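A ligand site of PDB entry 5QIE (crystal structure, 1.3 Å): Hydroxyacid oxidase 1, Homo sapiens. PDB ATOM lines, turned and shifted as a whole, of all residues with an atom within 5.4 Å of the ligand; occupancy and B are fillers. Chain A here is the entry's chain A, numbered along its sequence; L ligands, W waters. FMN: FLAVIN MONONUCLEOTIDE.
Tyr 27 touches the ligand.
Tyr 28 touches the ligand (CD1 to C7M, 3.3 Å).
Thr 81 touches the ligand (CA to C5A, 3.5 Å).
CE3 of Trp 111 touches O4 of the ligand, at 3.8 Å.
Gly 262 touches the ligand.
Arg 264 touches the ligand (NH2 to C7M, 3.4 Å).
Val 314 touches the ligand (C to O1P, 3.8 Å).
Hydrophobic or aromatic side chains that line the ligand: Tyr 27, Tyr 28, Ala 82, Trp 111, Tyr 133 and His 261.
Along chain A the residues within 4 Å of the ligand span positions 27 to 316.
The nearest printed residue that does not touch the ligand is Pro 317 (4.1 Å).
The side-chain amide nitrogen of Gln 131 sits close to the backbone NH of Tyr 133 (3.5 Å).
The guanidinium group (NE) of Arg 316 is in hydrogen-bond range of the backbone carbonyl oxygen (O) of Tyr 28 (2.8 Å).
OG of Ser 110 sits at hydrogen-bond distance from N of Tyr 133 (3.4 Å).
The backbone carbonyl oxygen of Val 314 sits at hydrogen-bond distance from the backbone NH of Gly 79 (2.9 Å).
The backbone NH of Ala 80 lies within hydrogen-bond range of the side-chain sulfur of Met 107.
O of Tyr 27 sits at hydrogen-bond distance from NH1 of Arg 264, at 2.8 Å.
N of His 261 sits at hydrogen-bond distance from OG of Ser 259 (3.0 Å).
The side-chain carboxylate (OD1) of Asp 292 sits at hydrogen-bond distance from the side-chain hydroxyl (OG) of Ser 259, at 2.7 Å.
Water W1 lies within hydrogen-bond range of an oxygen (O2P) of the ligand (2.8 Å), the side-chain amide nitrogen of Asn 41 (2.9 Å), the guanidinium group of Arg 316 (3.1 Å) and the backbone carbonyl oxygen of Gly 262 (3.5 Å).
Water W2 lies within hydrogen-bond range of OD2 of Asp 292 (2.8 Å) and O2' of the ligand (2.9 Å).
An oxygen (O5') of the ligand lies close to the backbone NH (N) of Gly 293, 3.5 Å away.
N of Gly 294 is in hydrogen-bond range of O2P of the ligand.
An oxygen (O3') of the ligand lies within hydrogen-bond range of the side-chain carboxylate (OD2) of Asp 292, 2.7 Å away.
N3 of the ligand lies within hydrogen-bond range of OH of Tyr 133.
N of Ala 82 lies within hydrogen-bond range of N5 of the ligand.
The side-chain hydroxyl of Thr 159 is in hydrogen-bond range of an oxygen (O2) of the ligand (2.7 Å).
NE2 of His 261 is in hydrogen-bond range of N1 of the ligand, 3.5 Å away.
An oxygen (O3') of the ligand lies within hydrogen-bond range of the side-chain hydroxyl of Ser 259 (3.3 Å).
NZ of Lys 237 is in hydrogen-bond range of O2 of the ligand, 2.9 Å away.
The guanidinium group of Arg 296 lies within salt-bridge range of an oxygen (O2P) of the ligand.
The side-chain amide oxygen (OE1) of Gln 131 lies within hydrogen-bond range of a nitrogen (N3) of the ligand (3.0 Å).
The backbone NH of Arg 316 lies within hydrogen-bond range of an oxygen (O3P) of the ligand, at 2.9 Å.
The side-chain hydroxyl of Ser 109 lies within hydrogen-bond range of an oxygen (O4) of the ligand (2.6 Å).
NH1 of Arg 316 is in salt-bridge range of O3P of the ligand, at 3.0 Å.
O2' of the ligand lies within hydrogen-bond range of O of Ala 80, at 2.7 Å.
O1P of the ligand is in hydrogen-bond range of N of Gly 315 (2.8 Å).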
ATOM      1  N   TYR A  27      21.882 -11.034  -5.366  1.00  0.00           N
ATOM      2  CA  TYR A  27      21.518 -11.630  -6.636  1.00  0.00           C
ATOM      3  C   TYR A  27      22.210 -10.901  -7.790  1.00  0.00           C
ATOM      4  O   TYR A  27      22.729 -11.475  -8.747  1.00  0.00           O
ATOM      5  CB  TYR A  27      19.976 -11.621  -6.818  1.00  0.00           C
ATOM      6  CG  TYR A  27      19.579 -11.895  -8.277  1.00  0.00           C
ATOM      7  CD1 TYR A  27      19.757 -13.135  -8.863  1.00  0.00           C
ATOM      8  CD2 TYR A  27      19.197 -10.839  -9.119  1.00  0.00           C
ATOM      9  CE1 TYR A  27      19.544 -13.330 -10.258  1.00  0.00           C
ATOM     10  CE2 TYR A  27      18.939 -11.028 -10.457  1.00  0.00           C
ATOM     11  CZ  TYR A  27      19.090 -12.279 -11.053  1.00  0.00           C
ATOM     12  OH  TYR A  27      18.935 -12.461 -12.400  1.00  0.00           O
ATOM     13  N   TYR A  28      22.133  -9.569  -7.736  1.00  0.00           N
ATOM     14  CA  TYR A  28      22.695  -8.752  -8.811  1.00  0.00           C
ATOM     15  C   TYR A  28      24.244  -8.780  -8.817  1.00  0.00           C
ATOM     16  O   TYR A  28      24.861  -8.800  -9.909  1.00  0.00           O
ATOM     17  CB  TYR A  28      22.189  -7.334  -8.661  1.00  0.00           C
ATOM     18  CG  TYR A  28      20.711  -7.078  -8.969  1.00  0.00           C
ATOM     19  CD1 TYR A  28      20.147  -7.513 -10.138  1.00  0.00           C
ATOM     20  CD2 TYR A  28      19.975  -6.206  -8.167  1.00  0.00           C
ATOM     21  CE1 TYR A  28      18.769  -7.208 -10.461  1.00  0.00           C
ATOM     22  CE2 TYR A  28      18.671  -5.829  -8.490  1.00  0.00           C
ATOM     23  CZ  TYR A  28      18.078  -6.358  -9.605  1.00  0.00           C
ATOM     24  OH  TYR A  28      16.782  -5.929  -9.942  1.00  0.00           O
ATOM     25  N   ASN A  41      37.293 -10.343 -14.542  1.00  0.00           N
ATOM     26  CA  ASN A  41      36.689  -9.467 -15.548  1.00  0.00           C
ATOM     27  C   ASN A  41      37.103  -8.037 -15.391  1.00  0.00           C
ATOM     28  O   ASN A  41      37.320  -7.356 -16.401  1.00  0.00           O
ATOM     29  CB  ASN A  41      35.160  -9.566 -15.558  1.00  0.00           C
ATOM     30  CG  ASN A  41      34.635 -10.745 -16.362  1.00  0.00           C
ATOM     31  OD1 ASN A  41      35.364 -11.458 -17.060  1.00  0.00           O
ATOM     32  ND2 ASN A  41      33.282 -10.965 -16.230  1.00  0.00           N
ATOM     33  N   GLY A  79      23.146  -4.236 -21.688  1.00  0.00           N
ATOM     34  CA  GLY A  79      22.998  -5.693 -21.739  1.00  0.00           C
ATOM     35  C   GLY A  79      21.781  -6.179 -20.954  1.00  0.00           C
ATOM     36  O   GLY A  79      21.281  -5.544 -20.022  1.00  0.00           O
ATOM     37  N   ALA A  80      21.370  -7.427 -21.280  1.00  0.00           N
ATOM     38  CA  ALA A  80      20.220  -8.071 -20.604  1.00  0.00           C
ATOM     39  C   ALA A  80      20.515  -8.341 -19.134  1.00  0.00           C
ATOM     40  O   ALA A  80      21.519  -9.030 -18.837  1.00  0.00           O
ATOM     41  CB  ALA A  80      19.825  -9.331 -21.304  1.00  0.00           C
ATOM     42  N   THR A  81      19.716  -7.846 -18.195  1.00  0.00           N
ATOM     43  CA  THR A  81      19.801  -8.181 -16.793  1.00  0.00           C
ATOM     44  C   THR A  81      18.395  -8.446 -16.343  1.00  0.00           C
ATOM     45  O   THR A  81      17.522  -7.583 -16.496  1.00  0.00           O
ATOM     46  CB  THR A  81      20.455  -7.111 -15.921  1.00  0.00           C
ATOM     47  OG1 THR A  81      19.884  -5.836 -16.221  1.00  0.00           O
ATOM     48  CG2 THR A  81      21.964  -7.031 -16.114  1.00  0.00           C
ATOM     49  N   ALA A  82      18.157  -9.660 -15.870  1.00  0.00           N
ATOM     50  CA  ALA A  82      16.821 -10.045 -15.518  1.00  0.00           C
ATOM     51  C   ALA A  82      16.209  -9.241 -14.361  1.00  0.00           C
ATOM     52  O   ALA A  82      16.881  -8.750 -13.487  1.00  0.00           O
ATOM     53  CB  ALA A  82      16.835 -11.500 -15.080  1.00  0.00           C
ATOM     54  N   MET A 107      19.212  -4.273 -24.774  1.00  0.00           N
ATOM     55  CA  MET A 107      18.963  -5.702 -24.885  1.00  0.00           C
ATOM     56  C   MET A 107      18.045  -6.158 -23.739  1.00  0.00           C
ATOM     57  O   MET A 107      18.383  -6.051 -22.568  1.00  0.00           O
ATOM     58  CB  MET A 107      20.287  -6.436 -24.836  1.00  0.00           C
ATOM     59  CG  MET A 107      20.165  -7.951 -25.146  1.00  0.00           C
ATOM     60  SD  MET A 107      21.550  -8.939 -24.555  1.00  0.00           S
ATOM     61  CE  MET A 107      22.921  -8.044 -25.326  1.00  0.00           C
ATOM     62  N   SER A 109      16.036  -8.707 -21.484  1.00  0.00           N
ATOM     63  CA  SER A 109      16.031 -10.075 -20.992  1.00  0.00           C
ATOM     64  C   SER A 109      14.740 -10.831 -21.249  1.00  0.00           C
ATOM     65  O   SER A 109      13.664 -10.288 -21.002  1.00  0.00           O
ATOM     66  CB  SER A 109      16.253 -10.014 -19.452  1.00  0.00           C
ATOM     67  OG  SER A 109      16.180 -11.328 -18.861  1.00  0.00           O
ATOM     68  N   SER A 110      14.874 -12.117 -21.572  1.00  0.00           N
ATOM     69  CA  SER A 110      13.651 -12.984 -21.615  1.00  0.00           C
ATOM     70  C   SER A 110      13.027 -13.091 -20.213  1.00  0.00           C
ATOM     71  O   SER A 110      11.822 -13.384 -20.040  1.00  0.00           O
ATOM     72  CB  SER A 110      13.991 -14.418 -22.135  1.00  0.00           C
ATOM     73  OG  SER A 110      14.122 -14.488 -23.520  1.00  0.00           O
ATOM     74  N   TRP A 111      13.828 -12.874 -19.189  1.00  0.00           N
ATOM     75  CA  TRP A 111      13.389 -12.938 -17.781  1.00  0.00           C
ATOM     76  C   TRP A 111      13.108 -11.564 -17.175  1.00  0.00           C
ATOM     77  O   TRP A 111      13.214 -11.347 -15.947  1.00  0.00           O
ATOM     78  CB  TRP A 111      14.509 -13.620 -16.938  1.00  0.00           C
ATOM     79  CG  TRP A 111      14.814 -15.022 -17.299  1.00  0.00           C
ATOM     80  CD1 TRP A 111      14.040 -15.871 -18.074  1.00  0.00           C
ATOM     81  CD2 TRP A 111      15.937 -15.826 -16.868  1.00  0.00           C
ATOM     82  NE1 TRP A 111      14.623 -17.110 -18.190  1.00  0.00           N
ATOM     83  CE2 TRP A 111      15.811 -17.084 -17.470  1.00  0.00           C
ATOM     84  CE3 TRP A 111      17.093 -15.552 -16.133  1.00  0.00           C
ATOM     85  CZ2 TRP A 111      16.789 -18.093 -17.296  1.00  0.00           C
ATOM     86  CZ3 TRP A 111      18.044 -16.567 -16.006  1.00  0.00           C
ATOM     87  CH2 TRP A 111      17.894 -17.767 -16.570  1.00  0.00           C
ATOM     88  N   GLN A 131      17.022 -10.536 -25.875  1.00  0.00           N
ATOM     89  CA  GLN A 131      17.833 -11.701 -25.448  1.00  0.00           C
ATOM     90  C   GLN A 131      16.878 -12.896 -25.231  1.00  0.00           C
ATOM     91  O   GLN A 131      15.876 -12.774 -24.495  1.00  0.00           O
ATOM     92  CB  GLN A 131      18.569 -11.379 -24.167  1.00  0.00           C
ATOM     93  CG  GLN A 131      19.345 -12.555 -23.601  1.00  0.00           C
ATOM     94  CD  GLN A 131      18.457 -13.437 -22.712  1.00  0.00           C
ATOM     95  OE1 GLN A 131      17.745 -12.932 -21.839  1.00  0.00           O
ATOM     96  NE2 GLN A 131      18.596 -14.772 -22.874  1.00  0.00           N
ATOM     97  N   TYR A 133      16.346 -16.974 -24.385  1.00  0.00           N
ATOM     98  CA  TYR A 133      16.642 -18.331 -23.864  1.00  0.00           C
ATOM     99  C   TYR A 133      15.794 -19.333 -24.646  1.00  0.00           C
ATOM    100  O   TYR A 133      14.633 -19.054 -24.981  1.00  0.00           O
ATOM    101  CB  TYR A 133      16.304 -18.405 -22.379  1.00  0.00           C
ATOM    102  CG  TYR A 133      17.343 -17.752 -21.473  1.00  0.00           C
ATOM    103  CD1 TYR A 133      18.629 -18.252 -21.408  1.00  0.00           C
ATOM    104  CD2 TYR A 133      17.027 -16.714 -20.603  1.00  0.00           C
ATOM    105  CE1 TYR A 133      19.557 -17.714 -20.576  1.00  0.00           C
ATOM    106  CE2 TYR A 133      17.954 -16.133 -19.751  1.00  0.00           C
ATOM    107  CZ  TYR A 133      19.223 -16.691 -19.732  1.00  0.00           C
ATOM    108  OH  TYR A 133      20.246 -16.216 -18.936  1.00  0.00           O
ATOM    109  N   THR A 159      21.238 -16.695 -25.931  1.00  0.00           N
ATOM    110  CA  THR A 159      22.205 -17.057 -24.879  1.00  0.00           C
ATOM    111  C   THR A 159      22.557 -18.510 -25.034  1.00  0.00           C
ATOM    112  O   THR A 159      21.650 -19.375 -25.050  1.00  0.00           O
ATOM    113  CB  THR A 159      21.668 -16.678 -23.511  1.00  0.00           C
ATOM    114  OG1 THR A 159      21.435 -15.253 -23.498  1.00  0.00           O
ATOM    115  CG2 THR A 159      22.645 -17.075 -22.418  1.00  0.00           C
ATOM    116  N   LYS A 237      25.406 -15.218 -27.897  1.00  0.00           N
ATOM    117  CA  LYS A 237      25.867 -14.574 -26.666  1.00  0.00           C
ATOM    118  C   LYS A 237      26.379 -15.611 -25.672  1.00  0.00           C
ATOM    119  O   LYS A 237      25.634 -16.520 -25.275  1.00  0.00           O
ATOM    120  CB  LYS A 237      24.685 -13.782 -26.045  1.00  0.00           C
ATOM    121  CG  LYS A 237      24.957 -13.214 -24.647  1.00  0.00           C
ATOM    122  CD  LYS A 237      23.788 -12.416 -24.069  1.00  0.00           C
ATOM    123  CE  LYS A 237      24.064 -11.711 -22.764  1.00  0.00           C
ATOM    124  NZ  LYS A 237      24.107 -12.672 -21.678  1.00  0.00           N
ATOM    125  N   SER A 259      31.274 -13.195 -24.013  1.00  0.00           N
ATOM    126  CA  SER A 259      30.640 -13.069 -22.734  1.00  0.00           C
ATOM    127  C   SER A 259      30.878 -14.305 -21.899  1.00  0.00           C
ATOM    128  O   SER A 259      30.827 -15.391 -22.454  1.00  0.00           O
ATOM    129  CB  SER A 259      29.120 -12.827 -22.882  1.00  0.00           C
ATOM    130  OG  SER A 259      28.457 -12.706 -21.674  1.00  0.00           O
ATOM    131  N   HIS A 261      28.861 -14.336 -19.189  1.00  0.00           N
ATOM    132  CA  HIS A 261      27.599 -14.157 -18.450  1.00  0.00           C
ATOM    133  C   HIS A 261      27.844 -13.378 -17.140  1.00  0.00           C
ATOM    134  O   HIS A 261      27.267 -13.691 -16.086  1.00  0.00           O
ATOM    135  CB  HIS A 261      26.931 -15.519 -18.195  1.00  0.00           C
ATOM    136  CG  HIS A 261      25.433 -15.493 -18.046  1.00  0.00           C
ATOM    137  ND1 HIS A 261      24.616 -16.233 -18.881  1.00  0.00           N
ATOM    138  CD2 HIS A 261      24.630 -14.899 -17.109  1.00  0.00           C
ATOM    139  CE1 HIS A 261      23.363 -16.074 -18.458  1.00  0.00           C
ATOM    140  NE2 HIS A 261      23.320 -15.273 -17.404  1.00  0.00           N
ATOM    141  N   GLY A 262      28.684 -12.336 -17.220  1.00  0.00           N
ATOM    142  CA  GLY A 262      28.973 -11.547 -16.008  1.00  0.00           C
ATOM    143  C   GLY A 262      29.645 -12.408 -14.926  1.00  0.00           C
ATOM    144  O   GLY A 262      29.484 -12.125 -13.748  1.00  0.00           O
ATOM    145  N   ARG A 264      28.858 -15.405 -14.049  1.00  0.00           N
ATOM    146  CA  ARG A 264      27.768 -16.042 -13.264  1.00  0.00           C
ATOM    147  C   ARG A 264      27.530 -17.481 -13.647  1.00  0.00           C
ATOM    148  O   ARG A 264      26.638 -18.102 -12.993  1.00  0.00           O
ATOM    149  CB  ARG A 264      26.485 -15.209 -13.410  1.00  0.00           C
ATOM    150  CG  ARG A 264      26.647 -13.802 -12.843  1.00  0.00           C
ATOM    151  CD  ARG A 264      25.642 -12.826 -13.346  1.00  0.00           C
ATOM    152  NE  ARG A 264      24.285 -13.057 -12.942  1.00  0.00           N
ATOM    153  CZ  ARG A 264      23.743 -12.581 -11.822  1.00  0.00           C
ATOM    154  NH1 ARG A 264      24.482 -11.983 -10.871  1.00  0.00           N
ATOM    155  NH2 ARG A 264      22.420 -12.633 -11.606  1.00  0.00           N
ATOM    156  N   ASP A 292      30.981  -8.125 -23.313  1.00  0.00           N
ATOM    157  CA  ASP A 292      30.492  -7.674 -22.030  1.00  0.00           C
ATOM    158  C   ASP A 292      31.346  -8.367 -20.940  1.00  0.00           C
ATOM    159  O   ASP A 292      32.107  -9.281 -21.235  1.00  0.00           O
ATOM    160  CB  ASP A 292      28.953  -7.842 -21.844  1.00  0.00           C
ATOM    161  CG  ASP A 292      28.480  -9.246 -21.771  1.00  0.00           C
ATOM    162  OD1 ASP A 292      29.211 -10.158 -21.391  1.00  0.00           O
ATOM    163  OD2 ASP A 292      27.259  -9.441 -22.062  1.00  0.00           O
ATOM    164  N   GLY A 293      31.163  -7.897 -19.710  1.00  0.00           N
ATOM    165  CA  GLY A 293      31.845  -8.472 -18.548  1.00  0.00           C
ATOM    166  C   GLY A 293      32.927  -7.490 -18.018  1.00  0.00           C
ATOM    167  O   GLY A 293      34.040  -7.442 -18.584  1.00  0.00           O
ATOM    168  N   GLY A 294      32.580  -6.798 -16.913  1.00  0.00           N
ATOM    169  CA  GLY A 294      33.586  -5.991 -16.265  1.00  0.00           C
ATOM    170  C   GLY A 294      33.738  -4.570 -16.784  1.00  0.00           C
ATOM    171  O   GLY A 294      34.620  -3.862 -16.316  1.00  0.00           O
ATOM    172  N   VAL A 295      32.899  -4.118 -17.723  1.00  0.00           N
ATOM    173  CA  VAL A 295      32.985  -2.738 -18.202  1.00  0.00           C
ATOM    174  C   VAL A 295      32.399  -1.793 -17.141  1.00  0.00           C
ATOM    175  O   VAL A 295      31.216  -1.826 -16.803  1.00  0.00           O
ATOM    176  CB  VAL A 295      32.255  -2.572 -19.548  1.00  0.00           C
ATOM    177  CG1 VAL A 295      32.255  -1.107 -19.971  1.00  0.00           C
ATOM    178  CG2 VAL A 295      32.832  -3.473 -20.630  1.00  0.00           C
ATOM    179  N   ARG A 296      33.279  -0.918 -16.626  1.00  0.00           N
ATOM    180  CA  ARG A 296      32.945   0.053 -15.601  1.00  0.00           C
ATOM    181  C   ARG A 296      33.422   1.477 -15.925  1.00  0.00           C
ATOM    182  O   ARG A 296      32.947   2.404 -15.247  1.00  0.00           O
ATOM    183  CB  ARG A 296      33.538  -0.352 -14.251  1.00  0.00           C
ATOM    184  CG  ARG A 296      33.232  -1.779 -13.770  1.00  0.00           C
ATOM    185  CD  ARG A 296      31.809  -1.959 -13.394  1.00  0.00           C
ATOM    186  NE  ARG A 296      31.528  -3.360 -13.040  1.00  0.00           N
ATOM    187  CZ  ARG A 296      30.929  -4.251 -13.818  1.00  0.00           C
ATOM    188  NH1 ARG A 296      30.558  -4.010 -15.047  1.00  0.00           N
ATOM    189  NH2 ARG A 296      30.725  -5.490 -13.319  1.00  0.00           N
ATOM    190  N   PHE A 313      28.627  -4.080 -24.047  1.00  0.00           N
ATOM    191  CA  PHE A 313      27.382  -4.063 -23.277  1.00  0.00           C
ATOM    192  C   PHE A 313      27.696  -3.984 -21.791  1.00  0.00           C
ATOM    193  O   PHE A 313      28.721  -4.577 -21.343  1.00  0.00           O
ATOM    194  CB  PHE A 313      26.524  -5.283 -23.553  1.00  0.00           C
ATOM    195  CG  PHE A 313      26.014  -5.353 -24.976  1.00  0.00           C
ATOM    196  CD1 PHE A 313      24.747  -4.899 -25.296  1.00  0.00           C
ATOM    197  CD2 PHE A 313      26.824  -5.770 -25.996  1.00  0.00           C
ATOM    198  CE1 PHE A 313      24.298  -4.912 -26.603  1.00  0.00           C
ATOM    199  CE2 PHE A 313      26.398  -5.741 -27.318  1.00  0.00           C
ATOM    200  CZ  PHE A 313      25.122  -5.320 -27.608  1.00  0.00           C
ATOM    201  N   VAL A 314      26.858  -3.237 -21.042  1.00  0.00           N
ATOM    202  CA  VAL A 314      26.951  -3.110 -19.589  1.00  0.00           C
ATOM    203  C   VAL A 314      25.815  -3.787 -18.919  1.00  0.00           C
ATOM    204  O   VAL A 314      24.646  -3.567 -19.354  1.00  0.00           O
ATOM    205  CB  VAL A 314      27.157  -1.672 -19.023  1.00  0.00           C
ATOM    206  CG1 VAL A 314      28.629  -1.254 -19.318  1.00  0.00           C
ATOM    207  CG2 VAL A 314      26.181  -0.741 -19.589  1.00  0.00           C
ATOM    208  N   GLY A 315      26.090  -4.590 -17.891  1.00  0.00           N
ATOM    209  CA  GLY A 315      25.063  -5.274 -17.140  1.00  0.00           C
ATOM    210  C   GLY A 315      24.815  -4.591 -15.830  1.00  0.00           C
ATOM    211  O   GLY A 315      23.927  -3.738 -15.682  1.00  0.00           O
ATOM    212  N   ARG A 316      25.597  -4.932 -14.818  1.00  0.00           N
ATOM    213  CA  ARG A 316      25.350  -4.489 -13.447  1.00  0.00           C
ATOM    214  C   ARG A 316      25.247  -2.948 -13.292  1.00  0.00           C
ATOM    215  O   ARG A 316      24.407  -2.491 -12.512  1.00  0.00           O
ATOM    216  CB  ARG A 316      26.382  -5.064 -12.474  1.00  0.00           C
ATOM    217  CG  ARG A 316      26.239  -6.538 -12.271  1.00  0.00           C
ATOM    218  CD  ARG A 316      27.320  -7.098 -11.385  1.00  0.00           C
ATOM    219  NE  ARG A 316      27.308  -8.572 -11.293  1.00  0.00           N
ATOM    220  CZ  ARG A 316      27.994  -9.367 -12.100  1.00  0.00           C
ATOM    221  NH1 ARG A 316      28.686  -8.914 -13.122  1.00  0.00           N
ATOM    222  NH2 ARG A 316      28.047 -10.652 -11.796  1.00  0.00           N
ATOM    223  N   PRO A 317      26.122  -2.175 -13.997  1.00  0.00           N
ATOM    224  CA  PRO A 317      26.017  -0.693 -13.775  1.00  0.00           C
ATOM    225  C   PRO A 317      24.608  -0.128 -14.006  1.00  0.00           C
ATOM    226  O   PRO A 317      24.188   0.801 -13.325  1.00  0.00           O
ATOM    227  CB  PRO A 317      27.012  -0.157 -14.782  1.00  0.00           C
ATOM    228  CG  PRO A 317      28.103  -1.235 -14.786  1.00  0.00           C
ATOM    229  CD  PRO A 317      27.302  -2.495 -14.832  1.00  0.00           C
ATOM    230  N   VAL A 319      21.716  -1.687 -13.451  1.00  0.00           N
ATOM    231  CA  VAL A 319      20.911  -2.043 -12.285  1.00  0.00           C
ATOM    232  C   VAL A 319      21.217  -1.113 -11.115  1.00  0.00           C
ATOM    233  O   VAL A 319      20.343  -0.687 -10.364  1.00  0.00           O
ATOM    234  CB  VAL A 319      21.137  -3.525 -11.908  1.00  0.00           C
ATOM    235  CG1 VAL A 319      20.417  -3.897 -10.647  1.00  0.00           C
ATOM    236  CG2 VAL A 319      20.738  -4.419 -13.078  1.00  0.00           C
HETATM  237  N1  FMN L   1      22.222 -12.725 -19.468  1.00  0.00           N
HETATM  238  C2  FMN L   1      21.170 -13.179 -20.205  1.00  0.00           C
HETATM  239  O2  FMN L   1      21.457 -13.682 -21.313  1.00  0.00           O
HETATM  240  N3  FMN L   1      19.904 -13.073 -19.722  1.00  0.00           N
HETATM  241  C4  FMN L   1      19.574 -12.621 -18.536  1.00  0.00           C
HETATM  242  O4  FMN L   1      18.398 -12.571 -18.118  1.00  0.00           O
HETATM  243  C4A FMN L   1      20.641 -12.125 -17.666  1.00  0.00           C
HETATM  244  N5  FMN L   1      20.390 -11.643 -16.450  1.00  0.00           N
HETATM  245  C5A FMN L   1      21.396 -11.121 -15.691  1.00  0.00           C
HETATM  246  C6  FMN L   1      21.118 -10.554 -14.425  1.00  0.00           C
HETATM  247  C7  FMN L   1      22.134  -9.984 -13.712  1.00  0.00           C
HETATM  248  C7M FMN L   1      21.794  -9.385 -12.371  1.00  0.00           C
HETATM  249  C8  FMN L   1      23.496  -9.993 -14.251  1.00  0.00           C
HETATM  250  C8M FMN L   1      24.588  -9.325 -13.383  1.00  0.00           C
HETATM  251  C9  FMN L   1      23.781 -10.505 -15.498  1.00  0.00           C
HETATM  252  C9A FMN L   1      22.772 -11.115 -16.251  1.00  0.00           C
HETATM  253  N10 FMN L   1      23.009 -11.674 -17.505  1.00  0.00           N
HETATM  254  C10 FMN L   1      21.955 -12.186 -18.269  1.00  0.00           C
HETATM  255  C1' FMN L   1      24.341 -11.569 -18.146  1.00  0.00           C
HETATM  256  C2' FMN L   1      24.444 -10.123 -18.710  1.00  0.00           C
HETATM  257  O2' FMN L   1      23.708 -10.023 -20.000  1.00  0.00           O
HETATM  258  C3' FMN L   1      25.869  -9.699 -19.066  1.00  0.00           C
HETATM  259  O3' FMN L   1      26.533 -10.777 -19.796  1.00  0.00           O
HETATM  260  C4' FMN L   1      26.689  -9.329 -17.818  1.00  0.00           C
HETATM  261  O4' FMN L   1      25.881  -8.602 -16.883  1.00  0.00           O
HETATM  262  C5' FMN L   1      27.892  -8.491 -18.220  1.00  0.00           C
HETATM  263  O5' FMN L   1      28.812  -8.242 -17.184  1.00  0.00           O
HETATM  264  P   FMN L   1      28.723  -6.934 -16.226  1.00  0.00           P
HETATM  265  O1P FMN L   1      28.568  -5.680 -17.061  1.00  0.00           O
HETATM  266  O2P FMN L   1      30.067  -6.985 -15.576  1.00  0.00           O
HETATM  267  O3P FMN L   1      27.581  -7.067 -15.270  1.00  0.00           O
HETATM  268  O   HOH W   1      31.310  -9.356 -14.756  1.00  0.00           O
HETATM  269  O   HOH W   2      24.713  -8.350 -22.175  1.00  0.00           O
HETATM  270  O   HOH W   3      30.252  -5.311 -19.048  1.00  0.00           O
